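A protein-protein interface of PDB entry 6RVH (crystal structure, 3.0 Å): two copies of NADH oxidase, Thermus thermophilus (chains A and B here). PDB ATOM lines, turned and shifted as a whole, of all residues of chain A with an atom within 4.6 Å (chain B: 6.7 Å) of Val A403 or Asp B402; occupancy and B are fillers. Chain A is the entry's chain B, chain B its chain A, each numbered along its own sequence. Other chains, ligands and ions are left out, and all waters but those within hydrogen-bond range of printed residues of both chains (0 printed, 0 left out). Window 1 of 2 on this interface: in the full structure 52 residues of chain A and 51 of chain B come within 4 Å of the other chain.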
ATOM      1  N   ARG A 400       4.508 -14.041 -16.852  1.00  0.00           N
ATOM      2  CA  ARG A 400       5.346 -14.718 -17.758  1.00  0.00           C
ATOM      3  C   ARG A 400       4.859 -16.130 -17.547  1.00  0.00           C
ATOM      4  O   ARG A 400       5.216 -17.034 -18.307  1.00  0.00           O
ATOM      5  CB  ARG A 400       6.761 -14.476 -17.234  1.00  0.00           C
ATOM      6  CG  ARG A 400       7.682 -13.979 -18.381  1.00  0.00           C
ATOM      7  CD  ARG A 400       8.969 -13.422 -17.813  1.00  0.00           C
ATOM      8  NE  ARG A 400       8.818 -12.172 -17.046  1.00  0.00           N
ATOM      9  CZ  ARG A 400       9.557 -11.090 -17.344  1.00  0.00           C
ATOM     10  NH1 ARG A 400      10.447 -11.088 -18.382  1.00  0.00           N
ATOM     11  NH2 ARG A 400       9.400 -10.006 -16.601  1.00  0.00           N
ATOM     12  N   ILE A 401       4.025 -16.330 -16.522  1.00  0.00           N
ATOM     13  CA  ILE A 401       3.643 -17.684 -16.181  1.00  0.00           C
ATOM     14  C   ILE A 401       2.914 -18.242 -17.323  1.00  0.00           C
ATOM     15  O   ILE A 401       2.826 -19.487 -17.450  1.00  0.00           O
ATOM     16  CB  ILE A 401       2.670 -17.718 -15.042  1.00  0.00           C
ATOM     17  CG1 ILE A 401       2.321 -19.160 -14.705  1.00  0.00           C
ATOM     18  CG2 ILE A 401       1.503 -16.973 -15.336  1.00  0.00           C
ATOM     19  CD1 ILE A 401       3.185 -19.705 -13.663  1.00  0.00           C
ATOM     20  N   ASP A 402       2.370 -17.303 -18.143  1.00  0.00           N
ATOM     21  CA  ASP A 402       1.342 -17.616 -19.173  1.00  0.00           C
ATOM     22  C   ASP A 402       2.057 -18.543 -20.200  1.00  0.00           C
ATOM     23  O   ASP A 402       1.459 -19.376 -20.848  1.00  0.00           O
ATOM     24  CB  ASP A 402       0.664 -16.296 -19.718  1.00  0.00           C
ATOM     25  CG  ASP A 402      -0.658 -15.888 -18.980  1.00  0.00           C
ATOM     26  OD1 ASP A 402      -1.249 -16.762 -18.317  1.00  0.00           O
ATOM     27  OD2 ASP A 402      -1.151 -14.723 -19.107  1.00  0.00           O
ATOM     28  N   VAL A 403       3.385 -18.441 -20.229  1.00  0.00           N
ATOM     29  CA  VAL A 403       4.210 -19.109 -21.269  1.00  0.00           C
ATOM     30  C   VAL A 403       4.265 -20.554 -20.895  1.00  0.00           C
ATOM     31  O   VAL A 403       4.226 -21.430 -21.734  1.00  0.00           O
ATOM     32  CB  VAL A 403       5.663 -18.493 -21.397  1.00  0.00           C
ATOM     33  CG1 VAL A 403       6.496 -19.332 -22.182  1.00  0.00           C
ATOM     34  CG2 VAL A 403       5.554 -17.193 -22.102  1.00  0.00           C
ATOM     35  N   LEU A 404       4.284 -20.777 -19.599  1.00  0.00           N
ATOM     36  CA  LEU A 404       4.548 -22.109 -19.058  1.00  0.00           C
ATOM     37  C   LEU A 404       3.308 -22.832 -19.324  1.00  0.00           C
ATOM     38  O   LEU A 404       3.354 -23.991 -19.775  1.00  0.00           O
ATOM     39  CB  LEU A 404       4.857 -22.127 -17.512  1.00  0.00           C
ATOM     40  CG  LEU A 404       6.195 -21.451 -17.109  1.00  0.00           C
ATOM     41  CD1 LEU A 404       6.443 -21.544 -15.658  1.00  0.00           C
ATOM     42  CD2 LEU A 404       7.302 -22.048 -17.896  1.00  0.00           C
ATOM     43  N   ALA A 405       2.213 -22.123 -19.052  1.00  0.00           N
ATOM     44  CA  ALA A 405       0.859 -22.653 -19.143  1.00  0.00           C
ATOM     45  C   ALA A 405       0.618 -23.125 -20.571  1.00  0.00           C
ATOM     46  O   ALA A 405      -0.025 -24.185 -20.793  1.00  0.00           O
ATOM     47  CB  ALA A 405      -0.095 -21.576 -18.747  1.00  0.00           C
ATOM     48  N   ALA A 406       1.146 -22.292 -21.504  1.00  0.00           N
ATOM     49  CA  ALA A 406       1.204 -22.503 -22.950  1.00  0.00           C
ATOM     50  C   ALA A 406       1.884 -23.846 -23.334  1.00  0.00           C
ATOM     51  O   ALA A 406       1.401 -24.644 -24.142  1.00  0.00           O
ATOM     52  CB  ALA A 406       1.961 -21.318 -23.553  1.00  0.00           C
ATOM     53  N   LEU A 407       3.074 -24.012 -22.764  1.00  0.00           N
ATOM     54  CA  LEU A 407       3.948 -25.158 -22.961  1.00  0.00           C
ATOM     55  C   LEU A 407       3.308 -26.286 -22.283  1.00  0.00           C
ATOM     56  O   LEU A 407       3.237 -27.305 -22.823  1.00  0.00           O
ATOM     57  CB  LEU A 407       5.288 -24.894 -22.308  1.00  0.00           C
ATOM     58  CG  LEU A 407       6.079 -24.021 -23.288  1.00  0.00           C
ATOM     59  CD1 LEU A 407       7.373 -23.644 -22.694  1.00  0.00           C
ATOM     60  CD2 LEU A 407       6.402 -24.791 -24.445  1.00  0.00           C
ATOM     61  N   LEU A 417      11.118 -24.737 -23.955  1.00  0.00           N
ATOM     62  CA  LEU A 417      11.081 -23.456 -23.300  1.00  0.00           C
ATOM     63  C   LEU A 417      12.331 -22.729 -23.684  1.00  0.00           C
ATOM     64  O   LEU A 417      12.338 -21.544 -23.921  1.00  0.00           O
ATOM     65  CB  LEU A 417      11.105 -23.659 -21.829  1.00  0.00           C
ATOM     66  CG  LEU A 417      11.133 -22.317 -21.056  1.00  0.00           C
ATOM     67  CD1 LEU A 417      10.125 -21.236 -21.411  1.00  0.00           C
ATOM     68  CD2 LEU A 417      10.893 -22.591 -19.621  1.00  0.00           C
ATOM     69  N   LEU A 420      12.549 -20.789 -27.159  1.00  0.00           N
ATOM     70  CA  LEU A 420      11.536 -19.750 -27.420  1.00  0.00           C
ATOM     71  C   LEU A 420      12.240 -18.517 -27.672  1.00  0.00           C
ATOM     72  O   LEU A 420      13.258 -18.270 -27.080  1.00  0.00           O
ATOM     73  CB  LEU A 420      10.504 -19.540 -26.327  1.00  0.00           C
ATOM     74  CG  LEU A 420       9.549 -20.710 -26.058  1.00  0.00           C
ATOM     75  CD1 LEU A 420       8.577 -20.233 -25.124  1.00  0.00           C
ATOM     76  CD2 LEU A 420       8.883 -21.188 -27.249  1.00  0.00           C
ATOM     77  N   LEU A 422      11.891 -15.112 -26.938  1.00  0.00           N
ATOM     78  CA  LEU A 422      11.209 -14.148 -26.127  1.00  0.00           C
ATOM     79  C   LEU A 422      11.558 -12.704 -26.382  1.00  0.00           C
ATOM     80  O   LEU A 422      12.439 -12.313 -27.180  1.00  0.00           O
ATOM     81  CB  LEU A 422      11.281 -14.526 -24.673  1.00  0.00           C
ATOM     82  CG  LEU A 422      10.940 -15.980 -24.328  1.00  0.00           C
ATOM     83  CD1 LEU A 422      10.882 -16.201 -22.851  1.00  0.00           C
ATOM     84  CD2 LEU A 422       9.670 -16.416 -24.871  1.00  0.00           C
ATOM     85  N   ALA A 423      10.758 -11.888 -25.715  1.00  0.00           N
ATOM     86  CA  ALA A 423      10.983 -10.449 -25.765  1.00  0.00           C
ATOM     87  C   ALA A 423      11.866  -9.900 -24.687  1.00  0.00           C
ATOM     88  O   ALA A 423      11.739 -10.290 -23.493  1.00  0.00           O
ATOM     89  CB  ALA A 423       9.745  -9.725 -25.777  1.00  0.00           C
ATOM     90  N   ASP A 433      15.631 -13.768 -20.692  1.00  0.00           N
ATOM     91  CA  ASP A 433      14.369 -13.882 -19.931  1.00  0.00           C
ATOM     92  C   ASP A 433      14.441 -14.896 -18.767  1.00  0.00           C
ATOM     93  O   ASP A 433      14.887 -15.983 -18.912  1.00  0.00           O
ATOM     94  CB  ASP A 433      13.124 -14.139 -20.800  1.00  0.00           C
ATOM     95  CG  ASP A 433      11.795 -13.732 -20.086  1.00  0.00           C
ATOM     96  OD1 ASP A 433      11.432 -14.530 -19.170  1.00  0.00           O
ATOM     97  OD2 ASP A 433      11.111 -12.675 -20.422  1.00  0.00           O
ATOM     98  N   LEU A 435      12.473 -16.921 -17.322  1.00  0.00           N
ATOM     99  CA  LEU A 435      12.178 -18.214 -17.938  1.00  0.00           C
ATOM    100  C   LEU A 435      13.379 -18.860 -18.687  1.00  0.00           C
ATOM    101  O   LEU A 435      13.650 -20.011 -18.503  1.00  0.00           O
ATOM    102  CB  LEU A 435      10.992 -18.084 -18.898  1.00  0.00           C
ATOM    103  CG  LEU A 435       9.746 -17.504 -18.296  1.00  0.00           C
ATOM    104  CD1 LEU A 435       8.861 -17.229 -19.400  1.00  0.00           C
ATOM    105  CD2 LEU A 435       9.163 -18.645 -17.428  1.00  0.00           C
ATOM    106  N   THR B 326      10.191 -11.944 -32.425  1.00  0.00           N
ATOM    107  CA  THR B 326       9.675 -11.223 -31.334  1.00  0.00           C
ATOM    108  C   THR B 326      10.455  -9.985 -30.963  1.00  0.00           C
ATOM    109  O   THR B 326      11.644 -10.070 -30.645  1.00  0.00           O
ATOM    110  CB  THR B 326       9.517 -12.209 -30.071  1.00  0.00           C
ATOM    111  OG1 THR B 326       8.808 -13.407 -30.462  1.00  0.00           O
ATOM    112  CG2 THR B 326       8.945 -11.482 -28.810  1.00  0.00           C
ATOM    113  N   THR B 339       5.592  -9.663 -33.057  1.00  0.00           N
ATOM    114  CA  THR B 339       6.125 -10.971 -33.238  1.00  0.00           C
ATOM    115  C   THR B 339       5.537 -11.579 -34.483  1.00  0.00           C
ATOM    116  O   THR B 339       4.378 -11.363 -34.863  1.00  0.00           O
ATOM    117  CB  THR B 339       5.834 -11.906 -31.974  1.00  0.00           C
ATOM    118  OG1 THR B 339       6.674 -13.047 -32.052  1.00  0.00           O
ATOM    119  CG2 THR B 339       4.289 -12.416 -31.669  1.00  0.00           C
ATOM    120  N   VAL B 391       1.074  -6.842 -29.103  1.00  0.00           N
ATOM    121  CA  VAL B 391       0.274  -6.486 -27.946  1.00  0.00           C
ATOM    122  C   VAL B 391       0.796  -5.200 -27.482  1.00  0.00           C
ATOM    123  O   VAL B 391       1.965  -5.006 -27.637  1.00  0.00           O
ATOM    124  CB  VAL B 391       0.108  -7.608 -26.791  1.00  0.00           C
ATOM    125  CG1 VAL B 391       0.760  -8.943 -27.152  1.00  0.00           C
ATOM    126  CG2 VAL B 391       0.447  -6.982 -25.403  1.00  0.00           C
ATOM    127  N   LEU B 399       3.529  -8.110 -22.962  1.00  0.00           N
ATOM    128  CA  LEU B 399       4.716  -9.022 -22.472  1.00  0.00           C
ATOM    129  C   LEU B 399       4.083 -10.413 -22.511  1.00  0.00           C
ATOM    130  O   LEU B 399       4.761 -11.454 -22.437  1.00  0.00           O
ATOM    131  CB  LEU B 399       5.192  -8.910 -21.002  1.00  0.00           C
ATOM    132  CG  LEU B 399       6.667  -9.340 -20.721  1.00  0.00           C
ATOM    133  CD1 LEU B 399       7.607  -8.993 -21.814  1.00  0.00           C
ATOM    134  CD2 LEU B 399       7.368  -8.692 -19.491  1.00  0.00           C
ATOM    135  N   ARG B 400       2.737 -10.320 -22.571  1.00  0.00           N
ATOM    136  CA  ARG B 400       1.820 -11.336 -22.984  1.00  0.00           C
ATOM    137  C   ARG B 400       2.240 -11.847 -24.460  1.00  0.00           C
ATOM    138  O   ARG B 400       1.814 -12.943 -24.956  1.00  0.00           O
ATOM    139  CB  ARG B 400       0.435 -10.666 -22.941  1.00  0.00           C
ATOM    140  CG  ARG B 400      -0.580 -11.436 -22.157  1.00  0.00           C
ATOM    141  CD  ARG B 400      -1.822 -10.683 -21.751  1.00  0.00           C
ATOM    142  NE  ARG B 400      -1.571  -9.500 -20.933  1.00  0.00           N
ATOM    143  CZ  ARG B 400      -2.258  -9.179 -19.835  1.00  0.00           C
ATOM    144  NH1 ARG B 400      -3.243  -9.997 -19.343  1.00  0.00           N
ATOM    145  NH2 ARG B 400      -1.921  -8.023 -19.222  1.00  0.00           N
ATOM    146  N   ILE B 401       3.054 -11.056 -25.161  1.00  0.00           N
ATOM    147  CA  ILE B 401       3.357 -11.367 -26.494  1.00  0.00           C
ATOM    148  C   ILE B 401       4.108 -12.743 -26.387  1.00  0.00           C
ATOM    149  O   ILE B 401       4.158 -13.583 -27.364  1.00  0.00           O
ATOM    150  CB  ILE B 401       4.243 -10.254 -26.977  1.00  0.00           C
ATOM    151  CG1 ILE B 401       4.704 -10.443 -28.392  1.00  0.00           C
ATOM    152  CG2 ILE B 401       5.455 -10.348 -26.325  1.00  0.00           C
ATOM    153  CD1 ILE B 401       3.748  -9.888 -29.352  1.00  0.00           C
ATOM    154  N   ASP B 402       4.689 -12.970 -25.189  1.00  0.00           N
ATOM    155  CA  ASP B 402       5.622 -14.042 -25.037  1.00  0.00           C
ATOM    156  C   ASP B 402       4.827 -15.247 -25.370  1.00  0.00           C
ATOM    157  O   ASP B 402       5.359 -16.233 -25.897  1.00  0.00           O
ATOM    158  CB  ASP B 402       6.403 -14.049 -23.696  1.00  0.00           C
ATOM    159  CG  ASP B 402       7.839 -13.272 -23.805  1.00  0.00           C
ATOM    160  OD1 ASP B 402       8.375 -12.969 -24.882  1.00  0.00           O
ATOM    161  OD2 ASP B 402       8.523 -12.882 -22.829  1.00  0.00           O
ATOM    162  N   VAL B 403       3.517 -15.165 -25.148  1.00  0.00           N
ATOM    163  CA  VAL B 403       2.682 -16.337 -25.384  1.00  0.00           C
ATOM    164  C   VAL B 403       2.546 -16.648 -26.872  1.00  0.00           C
ATOM    165  O   VAL B 403       2.681 -17.808 -27.339  1.00  0.00           O
ATOM    166  CB  VAL B 403       1.328 -16.269 -24.748  1.00  0.00           C
ATOM    167  CG1 VAL B 403       0.504 -17.431 -25.250  1.00  0.00           C
ATOM    168  CG2 VAL B 403       1.459 -16.335 -23.213  1.00  0.00           C
ATOM    169  N   LEU B 404       2.390 -15.586 -27.638  1.00  0.00           N
ATOM    170  CA  LEU B 404       2.192 -15.762 -29.049  1.00  0.00           C
ATOM    171  C   LEU B 404       3.451 -16.317 -29.675  1.00  0.00           C
ATOM    172  O   LEU B 404       3.406 -17.310 -30.430  1.00  0.00           O
ATOM    173  CB  LEU B 404       1.834 -14.446 -29.674  1.00  0.00           C
ATOM    174  CG  LEU B 404       0.505 -13.776 -29.335  1.00  0.00           C
ATOM    175  CD1 LEU B 404       0.359 -12.511 -30.115  1.00  0.00           C
ATOM    176  CD2 LEU B 404      -0.598 -14.658 -29.614  1.00  0.00           C
ATOM    177  N   ALA B 405       4.565 -15.667 -29.402  1.00  0.00           N
ATOM    178  CA  ALA B 405       5.842 -16.296 -29.664  1.00  0.00           C
ATOM    179  C   ALA B 405       5.984 -17.799 -29.404  1.00  0.00           C
ATOM    180  O   ALA B 405       6.575 -18.544 -30.218  1.00  0.00           O
ATOM    181  CB  ALA B 405       6.763 -15.671 -28.809  1.00  0.00           C
ATOM    182  N   ALA B 406       5.511 -18.192 -28.197  1.00  0.00           N
ATOM    183  CA  ALA B 406       5.435 -19.548 -27.787  1.00  0.00           C
ATOM    184  C   ALA B 406       4.622 -20.360 -28.741  1.00  0.00           C
ATOM    185  O   ALA B 406       5.024 -21.487 -29.045  1.00  0.00           O
ATOM    186  CB  ALA B 406       4.878 -19.626 -26.576  1.00  0.00           C
ATOM    187  N   LEU B 407       3.470 -19.834 -29.181  1.00  0.00           N
ATOM    188  CA  LEU B 407       2.550 -20.569 -30.081  1.00  0.00           C
ATOM    189  C   LEU B 407       3.063 -20.580 -31.422  1.00  0.00           C
ATOM    190  O   LEU B 407       2.907 -21.597 -32.074  1.00  0.00           O
ATOM    191  CB  LEU B 407       1.191 -19.930 -30.158  1.00  0.00           C
ATOM    192  CG  LEU B 407       0.451 -20.348 -28.905  1.00  0.00           C
ATOM    193  CD1 LEU B 407      -0.734 -19.496 -28.574  1.00  0.00           C
ATOM    194  CD2 LEU B 407       0.162 -21.814 -29.058  1.00  0.00           C
ATOM    195  N   LEU B 422      -4.941 -19.472 -19.162  1.00  0.00           N
ATOM    196  CA  LEU B 422      -4.221 -18.342 -18.605  1.00  0.00           C
ATOM    197  C   LEU B 422      -4.527 -17.876 -17.186  1.00  0.00           C
ATOM    198  O   LEU B 422      -5.494 -18.215 -16.559  1.00  0.00           O
ATOM    199  CB  LEU B 422      -4.254 -17.193 -19.572  1.00  0.00           C
ATOM    200  CG  LEU B 422      -3.933 -17.615 -21.001  1.00  0.00           C
ATOM    201  CD1 LEU B 422      -3.874 -16.429 -21.875  1.00  0.00           C
ATOM    202  CD2 LEU B 422      -2.639 -18.430 -21.149  1.00  0.00           C
ATOM    203  N   LEU B 435      -5.529 -11.690 -24.815  1.00  0.00           N
ATOM    204  CA  LEU B 435      -5.221 -12.807 -25.746  1.00  0.00           C
ATOM    205  C   LEU B 435      -6.429 -13.631 -26.022  1.00  0.00           C
ATOM    206  O   LEU B 435      -6.738 -13.809 -27.146  1.00  0.00           O
ATOM    207  CB  LEU B 435      -4.129 -13.705 -25.183  1.00  0.00           C
ATOM    208  CG  LEU B 435      -2.741 -13.058 -25.108  1.00  0.00           C
ATOM    209  CD1 LEU B 435      -1.719 -14.029 -24.441  1.00  0.00           C
ATOM    210  CD2 LEU B 435      -2.292 -12.518 -26.544  1.00  0.00           C
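The side-chain hydroxyl of Thr B326 sits at hydrogen-bond distance from the side-chain hydroxyl of Thr B339, 2.7 Å away. The side-chain carboxylate of Asp A433 lies within salt-bridge range of the guanidinium group of Arg A400 (2.7 Å). OD1 of Asp A433 lies close to N of Leu A435, at 3.2 Å.
Of the printed residues of chain B, Arg A400 touches Leu B399. Printed residues of chain B within 4 Å of Asp A402: Val B403 (3.6 Å) and Leu B422 (3.3 Å). Of chain B, only Asp B402 comes within 4 Å of Val A403. Asp B402 touches four residues of chain A. Of the printed residues of chain A, Val B403 touches Asp A402. Of the printed residues of chain A, Ala B406 touches Leu A420. The nearest residue of chain B that does not touch Val A403 is Val B403 (4.1 Å). The nearest printed residue of chain A that does not touch Leu B422 is Ala A405 (4.7 Å).
The side-chain carboxylate (OD1) of Asp B402 lies within hydrogen-bond range of the backbone NH (N) of Ala A423 (2.7 Å).
Asp A402 touches Val B403, and with the chains exchanged Val A403 touches Asp B402. Asp A402 touches Leu B422, and with the chains exchanged Leu A422 touches Asp B402. Of the 10 pairs that touch across the chains among the printed residues, 4 have their exchanged pair printed and touching as well.
Hydrophobic or aromatic side chains of chain A that line the printed part of chain B: Val A403, Leu A420, Leu A422 and Ala A423. Hydrophobic or aromatic side chains of chain B within 4 Å of the printed part of chain A: Leu B399, Val B403 and Leu B422. Among the printed residues, no Asp or Glu carboxylate lies within 4 Å of a Lys or Arg side-chain nitrogen of the other chain.
Among the printed residues, merely in contact across the chains: Arg A400 with Leu B399 (3.8 Å), Asp A402 with Val B403 (3.6 Å), Asp A402 with Leu B422 (3.3 Å), Val A403 with Asp B402 (3.6 Å), Leu A420 with Ala B406 (3.9 Å), Leu A422 with Thr B326 (3.8 Å), Leu A422 with Asp B402 (3.3 Å), Ala A423 with Thr B326 (3.6 Å) and Asp A433 with Asp B402 (3.5 Å).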
